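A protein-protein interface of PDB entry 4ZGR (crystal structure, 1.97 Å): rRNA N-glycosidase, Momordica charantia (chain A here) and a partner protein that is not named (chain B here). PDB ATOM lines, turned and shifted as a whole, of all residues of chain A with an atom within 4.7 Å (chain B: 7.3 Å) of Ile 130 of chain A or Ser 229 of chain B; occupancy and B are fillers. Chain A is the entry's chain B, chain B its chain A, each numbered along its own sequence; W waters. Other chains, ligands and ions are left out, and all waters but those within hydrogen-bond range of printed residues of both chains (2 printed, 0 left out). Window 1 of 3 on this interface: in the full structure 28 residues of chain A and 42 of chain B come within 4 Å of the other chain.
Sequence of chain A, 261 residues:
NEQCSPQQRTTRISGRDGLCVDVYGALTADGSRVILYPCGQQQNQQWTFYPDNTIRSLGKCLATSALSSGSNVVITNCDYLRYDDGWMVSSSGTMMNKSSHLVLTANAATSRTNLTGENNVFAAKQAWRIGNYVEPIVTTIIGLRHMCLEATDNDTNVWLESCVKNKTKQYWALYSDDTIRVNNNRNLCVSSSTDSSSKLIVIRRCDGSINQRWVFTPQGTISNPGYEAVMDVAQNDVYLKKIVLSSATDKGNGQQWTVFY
The side-chain hydroxyl (OH) of Tyr 231 of chain B lies within hydrogen-bond range of the backbone carbonyl oxygen (O) of Asn 208 of chain B, at 2.7 Å. The backbone NH (N) of Phe 211 of chain B sits at hydrogen-bond distance from the backbone carbonyl oxygen (O) of Asp 228 of chain B. OG of Ser 229 of chain B lies within hydrogen-bond range of N of Tyr 231 of chain B, at 3.1 Å. The backbone carbonyl oxygen (O) of Tyr 232 of chain B sits at hydrogen-bond distance from the side-chain hydroxyl (OG1) of Thr 236 of chain B (3.4 Å). The backbone NH of Gly 131 of chain A sits close to the side-chain hydroxyl of Thr 11 of chain A (3.5 Å). The backbone carbonyl oxygen (O) of Arg 12 of chain A is in hydrogen-bond range of the backbone NH (N) of Gly 131 of chain A (2.8 Å).
Of the 10 printed residues of chain A, 6 touch a printed residue of chain B. Hydrophobic or aromatic side chains of chain A within 4 Å of the printed part of chain B: Phe 49, Val 89 and Ile 130. Printed residues of chain B that touch a printed residue of chain A: Leu 207, Asn 208, Val 210, Asp 228, Ser 229, Tyr 231 and Tyr 232. Hydrophobic or aromatic side chains of chain B within 4 Å of the printed part of chain A: Leu 207, Val 210, Tyr 231 and Tyr 232. Among the printed residues, 12 pairs touch across the chains.
Among the printed residues, merely in contact across the chains: Phe 49 of chain A with Leu 207 of chain B (3.5 Å), Phe 49 of chain A with Val 210 of chain B (3.9 Å), Val 89 of chain A with Tyr 231 of chain B (3.2 Å), Arg 129 of chain A with Tyr 231 of chain B (3.6 Å), Arg 129 of chain A with Tyr 232 of chain B (3.7 Å), Ile 130 of chain A with Val 210 of chain B (3.5 Å), Ile 130 of chain A with Tyr 231 of chain B (3.7 Å), Gly 131 of chain A with Asp 228 of chain B (3.2 Å) and Gly 131 of chain A with Tyr 232 of chain B (3.3 Å).
Water W1 bridges the backbone carbonyl oxygen (O) of Tyr 231 of chain B and the guanidinium group (NE) of Arg 129 of chain A. Water W2 lies within hydrogen-bond range of the side-chain hydroxyl of Tyr 231 of chain B, the backbone carbonyl oxygen of Val 89 of chain A and the side-chain sulfur of Met 230 of chain B.
The side-chain amide oxygen of Asn 208 of chain B sits at hydrogen-bond distance from the backbone NH of Val 89 of chain A, 2.9 Å away. OD2 of Asp 228 of chain B lies within hydrogen-bond range of OG1 of Thr 11 of chain A (2.9 Å). OG of Ser 229 of chain B lies within hydrogen-bond range of O of Ile 130 of chain A, at 2.6 Å.
Printed residues of chain B within 4 Å of Ile 130 of chain A: Val 210 (3.5 Å), Ser 229 (2.6 Å) and Tyr 231 (3.7 Å). Printed residues of chain A within 4 Å of Ser 229 of chain B: Ile 130. Of the printed residues of chain A, Leu 207 of chain B touches Phe 49. Of the printed residues of chain A, Tyr 231 of chain B touches Val 89 (3.2 Å), Arg 129 (3.6 Å) and Ile 130 (3.7 Å). Of the printed residues of chain A, Asn 208 of chain B touches Val 89. Printed residues of chain A within 4 Å of Asp 228 of chain B: Thr 11 and Gly 131.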
ATOM      1  N   THR A  11     -24.466  18.621 -15.933  1.00  0.00           N
ATOM      2  CA  THR A  11     -23.725  17.965 -16.971  1.00  0.00           C
ATOM      3  C   THR A  11     -22.252  17.853 -16.545  1.00  0.00           C
ATOM      4  O   THR A  11     -21.902  18.304 -15.462  1.00  0.00           O
ATOM      5  CB  THR A  11     -23.875  18.757 -18.279  1.00  0.00           C
ATOM      6  OG1 THR A  11     -23.364  17.982 -19.356  1.00  0.00           O
ATOM      7  CG2 THR A  11     -23.151  20.068 -18.205  1.00  0.00           C
ATOM      8  N   ARG A  12     -21.406  17.255 -17.386  1.00  0.00           N
ATOM      9  CA  ARG A  12     -19.951  17.279 -17.155  1.00  0.00           C
ATOM     10  C   ARG A  12     -19.312  18.281 -18.111  1.00  0.00           C
ATOM     11  O   ARG A  12     -19.983  18.868 -18.977  1.00  0.00           O
ATOM     12  CB  ARG A  12     -19.340  15.890 -17.306  1.00  0.00           C
ATOM     13  CG  ARG A  12     -19.851  14.941 -16.237  1.00  0.00           C
ATOM     14  CD  ARG A  12     -19.192  13.589 -16.269  1.00  0.00           C
ATOM     15  NE  ARG A  12     -19.507  12.817 -17.457  1.00  0.00           N
ATOM     16  CZ  ARG A  12     -18.983  11.635 -17.723  1.00  0.00           C
ATOM     17  NH1 ARG A  12     -18.104  11.079 -16.899  1.00  0.00           N
ATOM     18  NH2 ARG A  12     -19.305  11.000 -18.825  1.00  0.00           N
ATOM     19  N   ILE A  13     -18.031  18.537 -17.898  1.00  0.00           N
ATOM     20  CA  ILE A  13     -17.282  19.425 -18.763  1.00  0.00           C
ATOM     21  C   ILE A  13     -15.945  18.780 -19.002  1.00  0.00           C
ATOM     22  O   ILE A  13     -15.201  18.533 -18.044  1.00  0.00           O
ATOM     23  CB  ILE A  13     -17.041  20.809 -18.146  1.00  0.00           C
ATOM     24  CG1 ILE A  13     -18.333  21.427 -17.631  1.00  0.00           C
ATOM     25  CG2 ILE A  13     -16.365  21.730 -19.167  1.00  0.00           C
ATOM     26  CD1 ILE A  13     -18.127  22.703 -16.844  1.00  0.00           C
ATOM     27  N   PHE A  49     -25.641  24.067 -14.554  1.00  0.00           N
ATOM     28  CA  PHE A  49     -25.780  25.359 -15.198  1.00  0.00           C
ATOM     29  C   PHE A  49     -27.141  25.964 -14.874  1.00  0.00           C
ATOM     30  O   PHE A  49     -28.154  25.266 -14.928  1.00  0.00           O
ATOM     31  CB  PHE A  49     -25.637  25.201 -16.709  1.00  0.00           C
ATOM     32  CG  PHE A  49     -24.230  24.918 -17.146  1.00  0.00           C
ATOM     33  CD1 PHE A  49     -23.670  23.671 -16.920  1.00  0.00           C
ATOM     34  CD2 PHE A  49     -23.473  25.883 -17.771  1.00  0.00           C
ATOM     35  CE1 PHE A  49     -22.370  23.397 -17.303  1.00  0.00           C
ATOM     36  CE2 PHE A  49     -22.175  25.620 -18.169  1.00  0.00           C
ATOM     37  CZ  PHE A  49     -21.624  24.367 -17.924  1.00  0.00           C
ATOM     38  N   VAL A  89     -20.185  31.228 -22.329  1.00  0.00           N
ATOM     39  CA  VAL A  89     -19.571  30.195 -23.124  1.00  0.00           C
ATOM     40  C   VAL A  89     -19.838  30.529 -24.592  1.00  0.00           C
ATOM     41  O   VAL A  89     -20.978  30.695 -24.985  1.00  0.00           O
ATOM     42  CB  VAL A  89     -20.132  28.812 -22.768  1.00  0.00           C
ATOM     43  CG1 VAL A  89     -19.406  27.723 -23.541  1.00  0.00           C
ATOM     44  CG2 VAL A  89     -20.024  28.572 -21.264  1.00  0.00           C
ATOM     45  N   MET A  95     -14.816  29.167 -22.456  1.00  0.00           N
ATOM     46  CA  MET A  95     -15.526  29.534 -21.239  1.00  0.00           C
ATOM     47  C   MET A  95     -14.879  30.772 -20.626  1.00  0.00           C
ATOM     48  O   MET A  95     -13.748  30.695 -20.104  1.00  0.00           O
ATOM     49  CB  MET A  95     -15.483  28.382 -20.254  1.00  0.00           C
ATOM     50  CG  MET A  95     -16.186  27.157 -20.795  1.00  0.00           C
ATOM     51  SD  MET A  95     -16.194  25.772 -19.658  1.00  0.00           S
ATOM     52  CE  MET A  95     -17.270  26.417 -18.376  1.00  0.00           C
ATOM     53  N   TRP A 128     -13.409  23.601 -24.611  1.00  0.00           N
ATOM     54  CA  TRP A 128     -14.137  22.693 -23.722  1.00  0.00           C
ATOM     55  C   TRP A 128     -15.425  22.249 -24.393  1.00  0.00           C
ATOM     56  O   TRP A 128     -16.033  23.019 -25.120  1.00  0.00           O
ATOM     57  CB  TRP A 128     -14.463  23.398 -22.402  1.00  0.00           C
ATOM     58  CG  TRP A 128     -13.231  23.962 -21.772  1.00  0.00           C
ATOM     59  CD1 TRP A 128     -12.709  25.220 -21.964  1.00  0.00           C
ATOM     60  CD2 TRP A 128     -12.312  23.276 -20.909  1.00  0.00           C
ATOM     61  NE1 TRP A 128     -11.517  25.347 -21.278  1.00  0.00           N
ATOM     62  CE2 TRP A 128     -11.263  24.179 -20.608  1.00  0.00           C
ATOM     63  CE3 TRP A 128     -12.281  21.996 -20.342  1.00  0.00           C
ATOM     64  CZ2 TRP A 128     -10.194  23.836 -19.763  1.00  0.00           C
ATOM     65  CZ3 TRP A 128     -11.213  21.653 -19.497  1.00  0.00           C
ATOM     66  CH2 TRP A 128     -10.187  22.569 -19.223  1.00  0.00           C
ATOM     67  N   ARG A 129     -15.811  21.011 -24.138  1.00  0.00           N
ATOM     68  CA  ARG A 129     -17.101  20.481 -24.459  1.00  0.00           C
ATOM     69  C   ARG A 129     -17.902  20.384 -23.158  1.00  0.00           C
ATOM     70  O   ARG A 129     -17.576  19.571 -22.256  1.00  0.00           O
ATOM     71  CB  ARG A 129     -16.967  19.103 -25.089  1.00  0.00           C
ATOM     72  CG  ARG A 129     -18.313  18.505 -25.470  1.00  0.00           C
ATOM     73  CD  ARG A 129     -18.250  17.028 -25.701  1.00  0.00           C
ATOM     74  NE  ARG A 129     -17.425  16.668 -26.833  1.00  0.00           N
ATOM     75  CZ  ARG A 129     -17.051  15.431 -27.116  1.00  0.00           C
ATOM     76  NH1 ARG A 129     -17.399  14.410 -26.322  1.00  0.00           N
ATOM     77  NH2 ARG A 129     -16.304  15.208 -28.176  1.00  0.00           N
ATOM     78  N   ILE A 130     -18.923  21.226 -23.043  1.00  0.00           N
ATOM     79  CA  ILE A 130     -19.910  21.082 -21.973  1.00  0.00           C
ATOM     80  C   ILE A 130     -20.897  20.007 -22.419  1.00  0.00           C
ATOM     81  O   ILE A 130     -21.572  20.154 -23.452  1.00  0.00           O
ATOM     82  CB  ILE A 130     -20.631  22.388 -21.683  1.00  0.00           C
ATOM     83  CG1 ILE A 130     -19.603  23.422 -21.235  1.00  0.00           C
ATOM     84  CG2 ILE A 130     -21.711  22.169 -20.613  1.00  0.00           C
ATOM     85  CD1 ILE A 130     -20.106  24.828 -21.145  1.00  0.00           C
ATOM     86  N   GLY A 131     -20.956  18.923 -21.654  1.00  0.00           N
ATOM     87  CA  GLY A 131     -21.805  17.808 -21.987  1.00  0.00           C
ATOM     88  C   GLY A 131     -21.503  16.533 -21.227  1.00  0.00           C
ATOM     89  O   GLY A 131     -20.360  16.261 -20.862  1.00  0.00           O
ATOM     90  N   LEU B 197     -34.495  18.642 -31.036  1.00  0.00           N
ATOM     91  CA  LEU B 197     -33.216  19.358 -31.170  1.00  0.00           C
ATOM     92  C   LEU B 197     -33.446  20.864 -31.404  1.00  0.00           C
ATOM     93  O   LEU B 197     -32.724  21.695 -30.866  1.00  0.00           O
ATOM     94  CB  LEU B 197     -32.372  18.769 -32.318  1.00  0.00           C
ATOM     95  CG  LEU B 197     -31.852  17.356 -32.088  1.00  0.00           C
ATOM     96  CD1 LEU B 197     -31.448  16.748 -33.416  1.00  0.00           C
ATOM     97  CD2 LEU B 197     -30.712  17.347 -31.081  1.00  0.00           C
ATOM     98  N   GLN B 200     -34.464  22.312 -27.992  1.00  0.00           N
ATOM     99  CA  GLN B 200     -33.328  22.393 -27.049  1.00  0.00           C
ATOM    100  C   GLN B 200     -32.271  23.432 -27.455  1.00  0.00           C
ATOM    101  O   GLN B 200     -31.817  24.205 -26.630  1.00  0.00           O
ATOM    102  CB  GLN B 200     -32.702  21.024 -26.812  1.00  0.00           C
ATOM    103  CG  GLN B 200     -33.639  19.985 -26.235  1.00  0.00           C
ATOM    104  CD  GLN B 200     -34.327  20.427 -24.955  1.00  0.00           C
ATOM    105  OE1 GLN B 200     -33.761  21.150 -24.145  1.00  0.00           O
ATOM    106  NE2 GLN B 200     -35.558  20.005 -24.780  1.00  0.00           N
ATOM    107  N   LEU B 201     -31.939  23.507 -28.737  1.00  0.00           N
ATOM    108  CA  LEU B 201     -31.005  24.529 -29.227  1.00  0.00           C
ATOM    109  C   LEU B 201     -31.459  25.945 -28.889  1.00  0.00           C
ATOM    110  O   LEU B 201     -30.689  26.750 -28.367  1.00  0.00           O
ATOM    111  CB  LEU B 201     -30.813  24.439 -30.733  1.00  0.00           C
ATOM    112  CG  LEU B 201     -29.821  23.410 -31.225  1.00  0.00           C
ATOM    113  CD1 LEU B 201     -30.041  23.123 -32.712  1.00  0.00           C
ATOM    114  CD2 LEU B 201     -28.395  23.874 -30.931  1.00  0.00           C
ATOM    115  N   SER B 204     -31.568  26.548 -25.147  1.00  0.00           N
ATOM    116  CA  SER B 204     -30.222  26.626 -24.580  1.00  0.00           C
ATOM    117  C   SER B 204     -29.593  28.011 -24.544  1.00  0.00           C
ATOM    118  O   SER B 204     -28.583  28.184 -23.882  1.00  0.00           O
ATOM    119  CB  SER B 204     -29.271  25.706 -25.323  1.00  0.00           C
ATOM    120  OG  SER B 204     -28.871  26.239 -26.570  1.00  0.00           O
ATOM    121  N   LEU B 207     -29.086  29.105 -21.042  1.00  0.00           N
ATOM    122  CA  LEU B 207     -28.277  28.241 -20.191  1.00  0.00           C
ATOM    123  C   LEU B 207     -26.901  28.025 -20.762  1.00  0.00           C
ATOM    124  O   LEU B 207     -26.390  26.914 -20.672  1.00  0.00           O
ATOM    125  CB  LEU B 207     -28.929  26.864 -20.015  1.00  0.00           C
ATOM    126  CG  LEU B 207     -29.867  26.486 -18.874  1.00  0.00           C
ATOM    127  CD1 LEU B 207     -29.947  24.967 -18.755  1.00  0.00           C
ATOM    128  CD2 LEU B 207     -29.462  27.107 -17.548  1.00  0.00           C
ATOM    129  N   ASN B 208     -26.280  29.068 -21.312  1.00  0.00           N
ATOM    130  CA  ASN B 208     -24.921  28.964 -21.850  1.00  0.00           C
ATOM    131  C   ASN B 208     -24.720  27.794 -22.824  1.00  0.00           C
ATOM    132  O   ASN B 208     -23.652  27.171 -22.873  1.00  0.00           O
ATOM    133  CB  ASN B 208     -23.902  28.898 -20.692  1.00  0.00           C
ATOM    134  CG  ASN B 208     -23.302  30.243 -20.372  1.00  0.00           C
ATOM    135  OD1 ASN B 208     -22.904  30.973 -21.271  1.00  0.00           O
ATOM    136  ND2 ASN B 208     -23.216  30.576 -19.100  1.00  0.00           N
ATOM    137  N   GLY B 209     -25.759  27.516 -23.617  1.00  0.00           N
ATOM    138  CA  GLY B 209     -25.679  26.505 -24.673  1.00  0.00           C
ATOM    139  C   GLY B 209     -25.961  25.098 -24.231  1.00  0.00           C
ATOM    140  O   GLY B 209     -25.848  24.179 -25.022  1.00  0.00           O
ATOM    141  N   VAL B 210     -26.390  24.935 -22.981  1.00  0.00           N
ATOM    142  CA  VAL B 210     -26.733  23.640 -22.430  1.00  0.00           C
ATOM    143  C   VAL B 210     -28.249  23.435 -22.594  1.00  0.00           C
ATOM    144  O   VAL B 210     -29.017  24.359 -22.415  1.00  0.00           O
ATOM    145  CB  VAL B 210     -26.330  23.579 -20.946  1.00  0.00           C
ATOM    146  CG1 VAL B 210     -26.733  22.259 -20.286  1.00  0.00           C
ATOM    147  CG2 VAL B 210     -24.817  23.790 -20.810  1.00  0.00           C
ATOM    148  N   PHE B 211     -28.641  22.211 -22.898  1.00  0.00           N
ATOM    149  CA  PHE B 211     -30.026  21.830 -23.135  1.00  0.00           C
ATOM    150  C   PHE B 211     -30.773  21.587 -21.815  1.00  0.00           C
ATOM    151  O   PHE B 211     -30.161  21.242 -20.790  1.00  0.00           O
ATOM    152  CB  PHE B 211     -30.057  20.521 -23.927  1.00  0.00           C
ATOM    153  CG  PHE B 211     -29.611  20.614 -25.370  1.00  0.00           C
ATOM    154  CD1 PHE B 211     -29.108  21.795 -25.949  1.00  0.00           C
ATOM    155  CD2 PHE B 211     -29.718  19.490 -26.172  1.00  0.00           C
ATOM    156  CE1 PHE B 211     -28.730  21.827 -27.275  1.00  0.00           C
ATOM    157  CE2 PHE B 211     -29.334  19.523 -27.516  1.00  0.00           C
ATOM    158  CZ  PHE B 211     -28.833  20.688 -28.062  1.00  0.00           C
ATOM    159  N   GLY B 212     -32.095  21.722 -21.846  1.00  0.00           N
ATOM    160  CA  GLY B 212     -32.947  21.265 -20.751  1.00  0.00           C
ATOM    161  C   GLY B 212     -33.092  19.769 -20.682  1.00  0.00           C
ATOM    162  O   GLY B 212     -33.342  19.205 -19.614  1.00  0.00           O
ATOM    163  N   ASP B 213     -32.960  19.104 -21.822  1.00  0.00           N
ATOM    164  CA  ASP B 213     -33.080  17.662 -21.891  1.00  0.00           C
ATOM    165  C   ASP B 213     -32.078  17.147 -22.891  1.00  0.00           C
ATOM    166  O   ASP B 213     -31.801  17.816 -23.893  1.00  0.00           O
ATOM    167  CB  ASP B 213     -34.498  17.248 -22.313  1.00  0.00           C
ATOM    168  CG  ASP B 213     -35.489  17.305 -21.159  1.00  0.00           C
ATOM    169  OD1 ASP B 213     -35.473  16.375 -20.316  1.00  0.00           O
ATOM    170  OD2 ASP B 213     -36.279  18.276 -21.079  1.00  0.00           O
ATOM    171  N   SER B 214     -31.561  15.951 -22.635  1.00  0.00           N
ATOM    172  CA  SER B 214     -30.610  15.309 -23.521  1.00  0.00           C
ATOM    173  C   SER B 214     -31.350  14.604 -24.650  1.00  0.00           C
ATOM    174  O   SER B 214     -32.464  14.098 -24.461  1.00  0.00           O
ATOM    175  CB  SER B 214     -29.739  14.321 -22.737  1.00  0.00           C
ATOM    176  OG  SER B 214     -28.776  13.713 -23.575  1.00  0.00           O
ATOM    177  N   VAL B 215     -30.742  14.598 -25.830  1.00  0.00           N
ATOM    178  CA  VAL B 215     -31.278  13.900 -26.993  1.00  0.00           C
ATOM    179  C   VAL B 215     -30.291  12.818 -27.376  1.00  0.00           C
ATOM    180  O   VAL B 215     -29.087  13.085 -27.458  1.00  0.00           O
ATOM    181  CB  VAL B 215     -31.493  14.899 -28.160  1.00  0.00           C
ATOM    182  CG1 VAL B 215     -31.911  14.186 -29.431  1.00  0.00           C
ATOM    183  CG2 VAL B 215     -32.498  15.975 -27.754  1.00  0.00           C
ATOM    184  N   GLY B 226     -25.195  10.981 -26.272  1.00  0.00           N
ATOM    185  CA  GLY B 226     -26.032  11.938 -25.564  1.00  0.00           C
ATOM    186  C   GLY B 226     -25.678  13.337 -26.009  1.00  0.00           C
ATOM    187  O   GLY B 226     -24.543  13.787 -25.833  1.00  0.00           O
ATOM    188  N   VAL B 227     -26.624  14.012 -26.640  1.00  0.00           N
ATOM    189  CA  VAL B 227     -26.445  15.396 -27.022  1.00  0.00           C
ATOM    190  C   VAL B 227     -27.283  16.248 -26.077  1.00  0.00           C
ATOM    191  O   VAL B 227     -28.517  16.313 -26.204  1.00  0.00           O
ATOM    192  CB  VAL B 227     -26.793  15.630 -28.505  1.00  0.00           C
ATOM    193  CG1 VAL B 227     -26.674  17.104 -28.851  1.00  0.00           C
ATOM    194  CG2 VAL B 227     -25.861  14.837 -29.392  1.00  0.00           C
ATOM    195  N   ASP B 228     -26.607  16.867 -25.103  1.00  0.00           N
ATOM    196  CA  ASP B 228     -27.259  17.682 -24.081  1.00  0.00           C
ATOM    197  C   ASP B 228     -26.764  19.130 -24.072  1.00  0.00           C
ATOM    198  O   ASP B 228     -26.909  19.843 -23.086  1.00  0.00           O
ATOM    199  CB  ASP B 228     -27.093  17.043 -22.698  1.00  0.00           C
ATOM    200  CG  ASP B 228     -25.629  16.973 -22.239  1.00  0.00           C
ATOM    201  OD1 ASP B 228     -24.714  17.053 -23.083  1.00  0.00           O
ATOM    202  OD2 ASP B 228     -25.404  16.795 -21.025  1.00  0.00           O
ATOM    203  N   SER B 229     -26.199  19.552 -25.195  1.00  0.00           N
ATOM    204  CA  SER B 229     -25.738  20.902 -25.396  1.00  0.00           C
ATOM    205  C   SER B 229     -25.499  21.109 -26.875  1.00  0.00           C
ATOM    206  O   SER B 229     -25.510  20.170 -27.669  1.00  0.00           O
ATOM    207  CB  SER B 229     -24.397  21.142 -24.667  1.00  0.00           C
ATOM    208  OG  SER B 229     -23.346  20.495 -25.368  1.00  0.00           O
ATOM    209  N   MET B 230     -25.198  22.348 -27.211  1.00  0.00           N
ATOM    210  CA  MET B 230     -24.817  22.708 -28.574  1.00  0.00           C
ATOM    211  C   MET B 230     -23.352  22.390 -28.938  1.00  0.00           C
ATOM    212  O   MET B 230     -22.942  22.684 -30.041  1.00  0.00           O
ATOM    213  CB  MET B 230     -25.062  24.193 -28.788  1.00  0.00           C
ATOM    214  CG  MET B 230     -24.118  25.105 -28.006  1.00  0.00           C
ATOM    215  SD  MET B 230     -24.289  26.851 -28.398  1.00  0.00           S
ATOM    216  CE  MET B 230     -23.565  26.904 -30.010  1.00  0.00           C
ATOM    217  N   TYR B 231     -22.572  21.801 -28.030  1.00  0.00           N
ATOM    218  CA  TYR B 231     -21.125  21.647 -28.236  1.00  0.00           C
ATOM    219  C   TYR B 231     -20.765  20.286 -28.830  1.00  0.00           C
ATOM    220  O   TYR B 231     -19.730  19.754 -28.512  1.00  0.00           O
ATOM    221  CB  TYR B 231     -20.409  21.954 -26.890  1.00  0.00           C
ATOM    222  CG  TYR B 231     -20.858  23.313 -26.347  1.00  0.00           C
ATOM    223  CD1 TYR B 231     -20.506  24.475 -27.011  1.00  0.00           C
ATOM    224  CD2 TYR B 231     -21.664  23.427 -25.219  1.00  0.00           C
ATOM    225  CE1 TYR B 231     -20.925  25.713 -26.575  1.00  0.00           C
ATOM    226  CE2 TYR B 231     -22.090  24.669 -24.760  1.00  0.00           C
ATOM    227  CZ  TYR B 231     -21.724  25.811 -25.460  1.00  0.00           C
ATOM    228  OH  TYR B 231     -22.106  27.048 -25.062  1.00  0.00           O
ATOM    229  N   TYR B 232     -21.646  19.697 -29.639  1.00  0.00           N
ATOM    230  CA  TYR B 232     -21.419  18.402 -30.292  1.00  0.00           C
ATOM    231  C   TYR B 232     -21.370  18.611 -31.810  1.00  0.00           C
ATOM    232  O   TYR B 232     -22.365  19.023 -32.389  1.00  0.00           O
ATOM    233  CB  TYR B 232     -22.514  17.394 -29.911  1.00  0.00           C
ATOM    234  CG  TYR B 232     -22.371  16.932 -28.488  1.00  0.00           C
ATOM    235  CD1 TYR B 232     -21.584  15.833 -28.183  1.00  0.00           C
ATOM    236  CD2 TYR B 232     -22.941  17.653 -27.434  1.00  0.00           C
ATOM    237  CE1 TYR B 232     -21.397  15.424 -26.873  1.00  0.00           C
ATOM    238  CE2 TYR B 232     -22.751  17.238 -26.107  1.00  0.00           C
ATOM    239  CZ  TYR B 232     -21.970  16.123 -25.844  1.00  0.00           C
ATOM    240  OH  TYR B 232     -21.761  15.682 -24.553  1.00  0.00           O
ATOM    241  N   LEU B 235     -24.164  17.400 -34.060  1.00  0.00           N
ATOM    242  CA  LEU B 235     -25.343  18.223 -34.159  1.00  0.00           C
ATOM    243  C   LEU B 235     -25.075  19.472 -35.001  1.00  0.00           C
ATOM    244  O   LEU B 235     -25.711  19.711 -36.022  1.00  0.00           O
ATOM    245  CB  LEU B 235     -25.833  18.656 -32.777  1.00  0.00           C
ATOM    246  CG  LEU B 235     -27.049  19.592 -32.771  1.00  0.00           C
ATOM    247  CD1 LEU B 235     -28.210  18.990 -33.558  1.00  0.00           C
ATOM    248  CD2 LEU B 235     -27.477  19.913 -31.353  1.00  0.00           C
ATOM    249  N   THR B 236     -24.128  20.266 -34.546  1.00  0.00           N
ATOM    250  CA  THR B 236     -24.030  21.626 -35.026  1.00  0.00           C
ATOM    251  C   THR B 236     -23.401  21.726 -36.428  1.00  0.00           C
ATOM    252  O   THR B 236     -23.665  22.682 -37.126  1.00  0.00           O
ATOM    253  CB  THR B 236     -23.393  22.546 -33.970  1.00  0.00           C
ATOM    254  OG1 THR B 236     -22.072  22.118 -33.713  1.00  0.00           O
ATOM    255  CG2 THR B 236     -24.180  22.507 -32.674  1.00  0.00           C
HETATM  256  O   HOH W   1     -17.187  18.966 -28.679  1.00  0.00           O
HETATM  257  O   HOH W   2     -22.845  29.188 -26.558  1.00  0.00           O
